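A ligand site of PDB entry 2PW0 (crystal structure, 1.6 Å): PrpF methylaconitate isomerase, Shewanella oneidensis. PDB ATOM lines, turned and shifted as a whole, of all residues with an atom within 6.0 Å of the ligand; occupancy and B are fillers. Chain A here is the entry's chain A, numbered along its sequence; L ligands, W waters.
OG of Ser 312 sits at hydrogen-bond distance from OG of Ser 69. The backbone NH of Lys 23 lies within hydrogen-bond range of the backbone carbonyl oxygen of Ser 70, at 2.9 Å. The side-chain amide nitrogen (ND2) of Asn 109 lies close to the backbone NH (N) of Gly 322. The backbone NH (N) of Asn 109 sits close to the side-chain sulfur (SG) of Cys 107 (3.4 Å). OD1 of Asn 109 sits at hydrogen-bond distance from N of Thr 21 (2.9 Å). NZ of Lys 281 sits at hydrogen-bond distance from ND1 of His 278 (2.9 Å). The backbone carbonyl oxygen of Ser 69 lies within hydrogen-bond range of the side-chain amide nitrogen of Gln 93 (2.8 Å). N of Leu 110 is in hydrogen-bond range of SG of Cys 107 (3.2 Å).
O of Ser 69 lies close to O5 of the ligand. His 278 touches the ligand (CE1 to O2, 3.4 Å). CE of Met 313 touches O1 of the ligand, at 3.6 Å. Met 321 touches the ligand (CA to O4, 3.3 Å). Hydrophobic or aromatic side chains within 4 Å of the ligand: His 278, Met 313, His 317 and Met 321.
Water W3 lies within hydrogen-bond range of O2 of the ligand (2.8 Å), OE1 of Gln 93 (2.8 Å) and NZ of Lys 73 (3.2 Å). Water W2 lies within hydrogen-bond range of the side-chain hydroxyl (OG1) of Thr 21, an oxygen (O4) of the ligand, the side-chain hydroxyl (OG) of Ser 22, a ring nitrogen (NE2) of His 317 and the side-chain amide nitrogen (ND2) of Asn 109. Water W4 lies within hydrogen-bond range of an oxygen (O2) of the ligand, the side-chain hydroxyl (OG1) of Thr 323 and the backbone carbonyl oxygen (O) of Asn 106.
O1 of the ligand is in hydrogen-bond range of OG of Ser 312 (2.5 Å). N of Ser 70 lies close to O6 of the ligand, 3.3 Å away. An oxygen (O6) of the ligand is in hydrogen-bond range of the side-chain hydroxyl (OG) of Ser 70 (2.6 Å). The side-chain hydroxyl (OG) of Ser 22 lies within hydrogen-bond range of an oxygen (O5) of the ligand. NZ of Lys 73 lies within salt-bridge range of O5 of the ligand, at 2.7 Å. The side-chain amide nitrogen (ND2) of Asn 109 is in hydrogen-bond range of an oxygen (O3) of the ligand (2.8 Å). O1 of the ligand is in salt-bridge range of NZ of Lys 281, at 2.8 Å. An oxygen (O6) of the ligand sits at hydrogen-bond distance from a ring nitrogen (NE2) of His 317 (2.8 Å). N of Gly 322 lies within hydrogen-bond range of O3 of the ligand, 2.8 Å away. The side-chain sulfur (SG) of Cys 107 lies within hydrogen-bond range of an oxygen (O3) of the ligand (3.7 Å).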
ATOM      1  N   THR A  21       4.470  -5.025  16.392  1.00  0.00           N
ATOM      2  CA  THR A  21       5.748  -4.359  16.162  1.00  0.00           C
ATOM      3  C   THR A  21       5.628  -3.208  15.152  1.00  0.00           C
ATOM      4  O   THR A  21       6.589  -2.910  14.448  1.00  0.00           O
ATOM      5  CB  THR A  21       6.820  -5.379  15.682  1.00  0.00           C
ATOM      6  OG1 THR A  21       6.375  -6.006  14.471  1.00  0.00           O
ATOM      7  CG2 THR A  21       7.032  -6.481  16.720  1.00  0.00           C
ATOM      8  N   SER A  22       4.447  -2.574  15.087  1.00  0.00           N
ATOM      9  CA  SER A  22       4.227  -1.434  14.194  1.00  0.00           C
ATOM     10  C   SER A  22       3.394  -0.352  14.909  1.00  0.00           C
ATOM     11  O   SER A  22       2.750  -0.614  15.933  1.00  0.00           O
ATOM     12  CB  SER A  22       3.510  -1.901  12.927  1.00  0.00           C
ATOM     13  OG  SER A  22       4.244  -2.905  12.231  1.00  0.00           O
ATOM     14  N   LYS A  23       3.397   0.860  14.339  1.00  0.00           N
ATOM     15  CA  LYS A  23       2.548   1.964  14.834  1.00  0.00           C
ATOM     16  C   LYS A  23       1.736   2.516  13.687  1.00  0.00           C
ATOM     17  O   LYS A  23       2.167   2.499  12.534  1.00  0.00           O
ATOM     18  CB  LYS A  23       3.406   3.116  15.372  1.00  0.00           C
ATOM     19  CG  LYS A  23       4.355   2.730  16.497  1.00  0.00           C
ATOM     20  CD  LYS A  23       5.015   3.975  17.145  1.00  0.00           C
ATOM     21  CE  LYS A  23       6.095   4.592  16.265  1.00  0.00           C
ATOM     22  NZ  LYS A  23       6.885   5.708  16.955  1.00  0.00           N
ATOM     23  N   SER A  69       8.325   1.548   6.853  1.00  0.00           N
ATOM     24  CA  SER A  69       7.085   0.830   6.561  1.00  0.00           C
ATOM     25  C   SER A  69       6.331   0.420   7.830  1.00  0.00           C
ATOM     26  O   SER A  69       5.145   0.137   7.767  1.00  0.00           O
ATOM     27  CB  SER A  69       7.332  -0.397   5.665  1.00  0.00           C
ATOM     28  OG  SER A  69       8.284  -1.260   6.265  1.00  0.00           O
ATOM     29  N   SER A  70       7.011   0.397   8.986  1.00  0.00           N
ATOM     30  CA  SER A  70       6.352   0.044  10.259  1.00  0.00           C
ATOM     31  C   SER A  70       5.719   1.225  10.953  1.00  0.00           C
ATOM     32  O   SER A  70       5.107   1.060  12.017  1.00  0.00           O
ATOM     33  CB  SER A  70       7.357  -0.567  11.251  1.00  0.00           C
ATOM     34  OG  SER A  70       8.004  -1.709  10.706  1.00  0.00           O
ATOM     35  N   THR A  71       5.867   2.413  10.373  1.00  0.00           N
ATOM     36  CA  THR A  71       5.354   3.624  11.015  1.00  0.00           C
ATOM     37  C   THR A  71       4.644   4.557  10.047  1.00  0.00           C
ATOM     38  O   THR A  71       4.148   5.610  10.463  1.00  0.00           O
ATOM     39  CB  THR A  71       6.499   4.424  11.682  1.00  0.00           C
ATOM     40  OG1 THR A  71       7.456   4.794  10.664  1.00  0.00           O
ATOM     41  CG2 THR A  71       7.183   3.627  12.777  1.00  0.00           C
ATOM     42  N   LYS A  73       1.618   4.409   8.364  1.00  0.00           N
ATOM     43  CA  LYS A  73       0.493   3.450   8.367  1.00  0.00           C
ATOM     44  C   LYS A  73      -0.788   4.067   8.861  1.00  0.00           C
ATOM     45  O   LYS A  73      -0.758   4.795   9.848  1.00  0.00           O
ATOM     46  CB  LYS A  73       0.840   2.247   9.261  1.00  0.00           C
ATOM     47  CG  LYS A  73       2.047   1.477   8.789  1.00  0.00           C
ATOM     48  CD  LYS A  73       2.479   0.414   9.797  1.00  0.00           C
ATOM     49  CE  LYS A  73       1.599  -0.813   9.730  1.00  0.00           C
ATOM     50  NZ  LYS A  73       2.022  -1.705   8.608  1.00  0.00           N
ATOM     51  N   PHE A  91      -6.949  -1.233   5.964  1.00  0.00           N
ATOM     52  CA  PHE A  91      -5.593  -0.852   6.246  1.00  0.00           C
ATOM     53  C   PHE A  91      -4.981  -0.120   5.039  1.00  0.00           C
ATOM     54  O   PHE A  91      -5.082  -0.598   3.903  1.00  0.00           O
ATOM     55  CB  PHE A  91      -4.708  -2.061   6.608  1.00  0.00           C
ATOM     56  CG  PHE A  91      -3.290  -1.689   6.714  1.00  0.00           C
ATOM     57  CD1 PHE A  91      -2.897  -0.770   7.700  1.00  0.00           C
ATOM     58  CD2 PHE A  91      -2.356  -2.117   5.782  1.00  0.00           C
ATOM     59  CE1 PHE A  91      -1.582  -0.346   7.778  1.00  0.00           C
ATOM     60  CE2 PHE A  91      -1.018  -1.711   5.866  1.00  0.00           C
ATOM     61  CZ  PHE A  91      -0.653  -0.812   6.863  1.00  0.00           C
ATOM     62  N   GLN A  93      -1.348   1.334   3.696  1.00  0.00           N
ATOM     63  CA  GLN A  93       0.090   1.473   3.786  1.00  0.00           C
ATOM     64  C   GLN A  93       0.508   2.721   3.000  1.00  0.00           C
ATOM     65  O   GLN A  93       0.403   2.746   1.773  1.00  0.00           O
ATOM     66  CB  GLN A  93       0.818   0.234   3.231  1.00  0.00           C
ATOM     67  CG  GLN A  93       2.328   0.234   3.477  1.00  0.00           C
ATOM     68  CD  GLN A  93       2.719   0.042   4.945  1.00  0.00           C
ATOM     69  OE1 GLN A  93       2.103  -0.751   5.655  1.00  0.00           O
ATOM     70  NE2 GLN A  93       3.748   0.780   5.403  1.00  0.00           N
ATOM     71  N   ASN A 106      -3.471  -6.546   4.134  1.00  0.00           N
ATOM     72  CA  ASN A 106      -3.739  -6.417   5.548  1.00  0.00           C
ATOM     73  C   ASN A 106      -2.439  -6.079   6.254  1.00  0.00           C
ATOM     74  O   ASN A 106      -1.352  -6.388   5.723  1.00  0.00           O
ATOM     75  CB  ASN A 106      -4.237  -7.773   6.068  1.00  0.00           C
ATOM     76  CG  ASN A 106      -4.541  -7.777   7.564  1.00  0.00           C
ATOM     77  OD1 ASN A 106      -4.915  -6.758   8.138  1.00  0.00           O
ATOM     78  ND2 ASN A 106      -4.414  -8.955   8.186  1.00  0.00           N
ATOM     79  N   CYS A 107      -2.541  -5.437   7.419  1.00  0.00           N
ATOM     80  CA  CYS A 107      -1.392  -5.373   8.336  1.00  0.00           C
ATOM     81  C   CYS A 107      -1.676  -6.318   9.472  1.00  0.00           C
ATOM     82  O   CYS A 107      -2.578  -6.074  10.293  1.00  0.00           O
ATOM     83  CB  CYS A 107      -1.131  -3.986   8.917  1.00  0.00           C
ATOM     84  SG  CYS A 107       0.345  -4.061  10.038  1.00  0.00           S
ATOM     85  N   GLY A 108      -0.921  -7.412   9.520  1.00  0.00           N
ATOM     86  CA  GLY A 108      -1.082  -8.390  10.581  1.00  0.00           C
ATOM     87  C   GLY A 108      -0.522  -7.980  11.946  1.00  0.00           C
ATOM     88  O   GLY A 108      -0.793  -8.650  12.934  1.00  0.00           O
ATOM     89  N   ASN A 109       0.239  -6.894  11.995  1.00  0.00           N
ATOM     90  CA  ASN A 109       0.658  -6.329  13.286  1.00  0.00           C
ATOM     91  C   ASN A 109      -0.386  -5.372  13.819  1.00  0.00           C
ATOM     92  O   ASN A 109      -0.785  -5.480  15.000  1.00  0.00           O
ATOM     93  CB  ASN A 109       2.032  -5.655  13.163  1.00  0.00           C
ATOM     94  CG  ASN A 109       3.153  -6.609  13.523  1.00  0.00           C
ATOM     95  OD1 ASN A 109       3.273  -7.036  14.675  1.00  0.00           O
ATOM     96  ND2 ASN A 109       3.964  -6.979  12.536  1.00  0.00           N
ATOM     97  N   LEU A 110      -0.834  -4.418  12.990  1.00  0.00           N
ATOM     98  CA  LEU A 110      -1.903  -3.524  13.508  1.00  0.00           C
ATOM     99  C   LEU A 110      -3.222  -4.244  13.811  1.00  0.00           C
ATOM    100  O   LEU A 110      -4.077  -3.735  14.560  1.00  0.00           O
ATOM    101  CB  LEU A 110      -2.119  -2.292  12.632  1.00  0.00           C
ATOM    102  CG  LEU A 110      -0.908  -1.364  12.503  1.00  0.00           C
ATOM    103  CD1 LEU A 110      -1.291  -0.077  11.734  1.00  0.00           C
ATOM    104  CD2 LEU A 110      -0.357  -1.045  13.872  1.00  0.00           C
ATOM    105  N   ILE A 222      -0.575 -12.933   3.106  1.00  0.00           N
ATOM    106  CA  ILE A 222      -0.263 -12.009   2.028  1.00  0.00           C
ATOM    107  C   ILE A 222       0.449 -12.885   0.994  1.00  0.00           C
ATOM    108  O   ILE A 222       1.040 -13.907   1.367  1.00  0.00           O
ATOM    109  CB  ILE A 222       0.642 -10.827   2.547  1.00  0.00           C
ATOM    110  CG1 ILE A 222       0.626  -9.636   1.574  1.00  0.00           C
ATOM    111  CG2 ILE A 222       2.058 -11.302   2.909  1.00  0.00           C
ATOM    112  CD1 ILE A 222       0.889  -8.266   2.262  1.00  0.00           C
ATOM    113  N   HIS A 278       4.102  -3.560  -2.728  1.00  0.00           N
ATOM    114  CA  HIS A 278       3.567  -4.099  -1.467  1.00  0.00           C
ATOM    115  C   HIS A 278       3.360  -5.623  -1.539  1.00  0.00           C
ATOM    116  O   HIS A 278       3.601  -6.326  -0.555  1.00  0.00           O
ATOM    117  CB  HIS A 278       2.287  -3.352  -1.064  1.00  0.00           C
ATOM    118  CG  HIS A 278       1.837  -3.586   0.351  1.00  0.00           C
ATOM    119  ND1 HIS A 278       2.707  -3.845   1.398  1.00  0.00           N
ATOM    120  CD2 HIS A 278       0.601  -3.566   0.894  1.00  0.00           C
ATOM    121  CE1 HIS A 278       2.017  -3.997   2.515  1.00  0.00           C
ATOM    122  NE2 HIS A 278       0.737  -3.827   2.239  1.00  0.00           N
ATOM    123  N   LYS A 281       5.327 -10.325  -1.178  1.00  0.00           N
ATOM    124  CA  LYS A 281       6.480 -10.146  -0.311  1.00  0.00           C
ATOM    125  C   LYS A 281       7.504 -11.180  -0.711  1.00  0.00           C
ATOM    126  O   LYS A 281       7.143 -12.225  -1.257  1.00  0.00           O
ATOM    127  CB  LYS A 281       6.110 -10.369   1.162  1.00  0.00           C
ATOM    128  CG  LYS A 281       5.062  -9.409   1.718  1.00  0.00           C
ATOM    129  CD  LYS A 281       5.511  -7.942   1.555  1.00  0.00           C
ATOM    130  CE  LYS A 281       4.599  -6.990   2.313  1.00  0.00           C
ATOM    131  NZ  LYS A 281       4.925  -5.580   1.985  1.00  0.00           N
ATOM    132  N   LEU A 311      11.693  -9.120   3.292  1.00  0.00           N
ATOM    133  CA  LEU A 311      11.830  -7.762   2.787  1.00  0.00           C
ATOM    134  C   LEU A 311      10.493  -7.051   2.833  1.00  0.00           C
ATOM    135  O   LEU A 311       9.435  -7.648   2.627  1.00  0.00           O
ATOM    136  CB  LEU A 311      12.376  -7.756   1.364  1.00  0.00           C
ATOM    137  CG  LEU A 311      13.888  -7.958   1.269  1.00  0.00           C
ATOM    138  CD1 LEU A 311      14.271  -9.431   1.347  1.00  0.00           C
ATOM    139  CD2 LEU A 311      14.399  -7.329   0.002  1.00  0.00           C
ATOM    140  N   SER A 312      10.556  -5.743   3.106  1.00  0.00           N
ATOM    141  CA  SER A 312       9.389  -4.901   3.165  1.00  0.00           C
ATOM    142  C   SER A 312       9.713  -3.618   2.381  1.00  0.00           C
ATOM    143  O   SER A 312      10.599  -2.854   2.785  1.00  0.00           O
ATOM    144  CB  SER A 312       9.079  -4.567   4.627  1.00  0.00           C
ATOM    145  OG  SER A 312       8.135  -3.528   4.707  1.00  0.00           O
ATOM    146  N   MET A 313       9.004  -3.398   1.280  1.00  0.00           N
ATOM    147  CA  MET A 313       9.243  -2.250   0.415  1.00  0.00           C
ATOM    148  C   MET A 313      10.700  -2.108   0.024  1.00  0.00           C
ATOM    149  O   MET A 313      11.274  -0.999   0.011  1.00  0.00           O
ATOM    150  CB  MET A 313       8.672  -0.973   1.044  1.00  0.00           C
ATOM    151  CG  MET A 313       7.324  -0.613   0.456  1.00  0.00           C
ATOM    152  SD  MET A 313       6.057  -1.845   0.761  1.00  0.00           S
ATOM    153  CE  MET A 313       5.799  -1.633   2.519  1.00  0.00           C
ATOM    154  N   HIS A 317      13.231  -6.267   6.539  1.00  0.00           N
ATOM    155  CA  HIS A 317      12.350  -5.876   7.640  1.00  0.00           C
ATOM    156  C   HIS A 317      13.041  -6.056   8.994  1.00  0.00           C
ATOM    157  O   HIS A 317      13.808  -6.979   9.194  1.00  0.00           O
ATOM    158  CB  HIS A 317      11.038  -6.691   7.584  1.00  0.00           C
ATOM    159  CG  HIS A 317       9.947  -6.148   8.453  1.00  0.00           C
ATOM    160  ND1 HIS A 317       9.746  -6.565   9.754  1.00  0.00           N
ATOM    161  CD2 HIS A 317       8.987  -5.222   8.206  1.00  0.00           C
ATOM    162  CE1 HIS A 317       8.711  -5.922  10.265  1.00  0.00           C
ATOM    163  NE2 HIS A 317       8.237  -5.102   9.346  1.00  0.00           N
ATOM    164  N   HIS A 318      12.726  -5.152   9.924  1.00  0.00           N
ATOM    165  CA  HIS A 318      13.367  -5.139  11.224  1.00  0.00           C
ATOM    166  C   HIS A 318      12.997  -6.328  12.136  1.00  0.00           C
ATOM    167  O   HIS A 318      13.734  -6.660  13.054  1.00  0.00           O
ATOM    168  CB  HIS A 318      13.077  -3.808  11.918  1.00  0.00           C
ATOM    169  CG  HIS A 318      11.700  -3.708  12.515  1.00  0.00           C
ATOM    170  ND1 HIS A 318      10.566  -3.489  11.765  1.00  0.00           N
ATOM    171  CD2 HIS A 318      11.291  -3.785  13.800  1.00  0.00           C
ATOM    172  CE1 HIS A 318       9.513  -3.437  12.564  1.00  0.00           C
ATOM    173  NE2 HIS A 318       9.928  -3.616  13.802  1.00  0.00           N
ATOM    174  N   MET A 320       9.390  -9.244  11.755  1.00  0.00           N
ATOM    175  CA  MET A 320       8.672  -9.987  10.706  1.00  0.00           C
ATOM    176  C   MET A 320       7.263  -9.437  10.543  1.00  0.00           C
ATOM    177  O   MET A 320       6.567  -9.203  11.524  1.00  0.00           O
ATOM    178  CB  MET A 320       8.619 -11.473  11.035  1.00  0.00           C
ATOM    179  CG  MET A 320       7.977 -12.310   9.923  1.00  0.00           C
ATOM    180  SD  MET A 320       8.790 -12.140   8.323  1.00  0.00           S
ATOM    181  CE  MET A 320      10.425 -12.712   8.779  1.00  0.00           C
ATOM    182  N   MET A 321       6.835  -9.250   9.297  1.00  0.00           N
ATOM    183  CA  MET A 321       5.508  -8.715   9.058  1.00  0.00           C
ATOM    184  C   MET A 321       4.494  -9.739   9.552  1.00  0.00           C
ATOM    185  O   MET A 321       4.738 -10.937   9.466  1.00  0.00           O
ATOM    186  CB  MET A 321       5.298  -8.435   7.575  1.00  0.00           C
ATOM    187  CG  MET A 321       6.255  -7.390   7.032  1.00  0.00           C
ATOM    188  SD  MET A 321       7.798  -8.038   6.335  1.00  0.00           S
ATOM    189  CE  MET A 321       7.190  -8.745   4.794  1.00  0.00           C
ATOM    190  N   GLY A 322       3.381  -9.266  10.111  1.00  0.00           N
ATOM    191  CA  GLY A 322       2.375 -10.170  10.670  1.00  0.00           C
ATOM    192  C   GLY A 322       1.770 -11.059   9.608  1.00  0.00           C
ATOM    193  O   GLY A 322       1.493 -12.243   9.868  1.00  0.00           O
ATOM    194  N   THR A 323       1.535 -10.500   8.431  1.00  0.00           N
ATOM    195  CA  THR A 323       1.005 -11.292   7.311  1.00  0.00           C
ATOM    196  C   THR A 323       2.015 -12.368   6.899  1.00  0.00           C
ATOM    197  O   THR A 323       1.646 -13.515   6.591  1.00  0.00           O
ATOM    198  CB  THR A 323       0.738 -10.428   6.080  1.00  0.00           C
ATOM    199  OG1 THR A 323       1.913  -9.688   5.755  1.00  0.00           O
ATOM    200  CG2 THR A 323      -0.457  -9.504   6.327  1.00  0.00           C
HETATM  201  C1  LIG L   1       5.005  -4.539   5.329  1.00  0.00           C
HETATM  202  O1  LIG L   1       5.893  -4.631   4.437  1.00  0.00           O
HETATM  203  O2  LIG L   1       3.850  -5.038   5.223  1.00  0.00           O
HETATM  204  C2  LIG L   1       5.339  -3.824   6.488  1.00  0.00           C
HETATM  205  C3  LIG L   1       4.762  -3.960   7.769  1.00  0.00           C
HETATM  206  C4  LIG L   1       3.671  -4.981   8.149  1.00  0.00           C
HETATM  207  C5  LIG L   1       4.043  -5.719   9.457  1.00  0.00           C
HETATM  208  O3  LIG L   1       3.142  -6.432   9.958  1.00  0.00           O
HETATM  209  O4  LIG L   1       5.183  -5.547   9.940  1.00  0.00           O
HETATM  210  C6  LIG L   1       5.257  -3.050   8.883  1.00  0.00           C
HETATM  211  O5  LIG L   1       4.389  -2.541   9.626  1.00  0.00           O
HETATM  212  O6  LIG L   1       6.481  -2.889   8.994  1.00  0.00           O
HETATM  213  O   HOH W   1       1.563  -7.544   8.169  1.00  0.00           O
HETATM  214  O   HOH W   2       6.505  -4.605  12.179  1.00  0.00           O
HETATM  215  O   HOH W   3       1.730  -3.463   5.999  1.00  0.00           O
HETATM  216  O   HOH W   4       1.631  -6.805   5.535  1.00  0.00           O
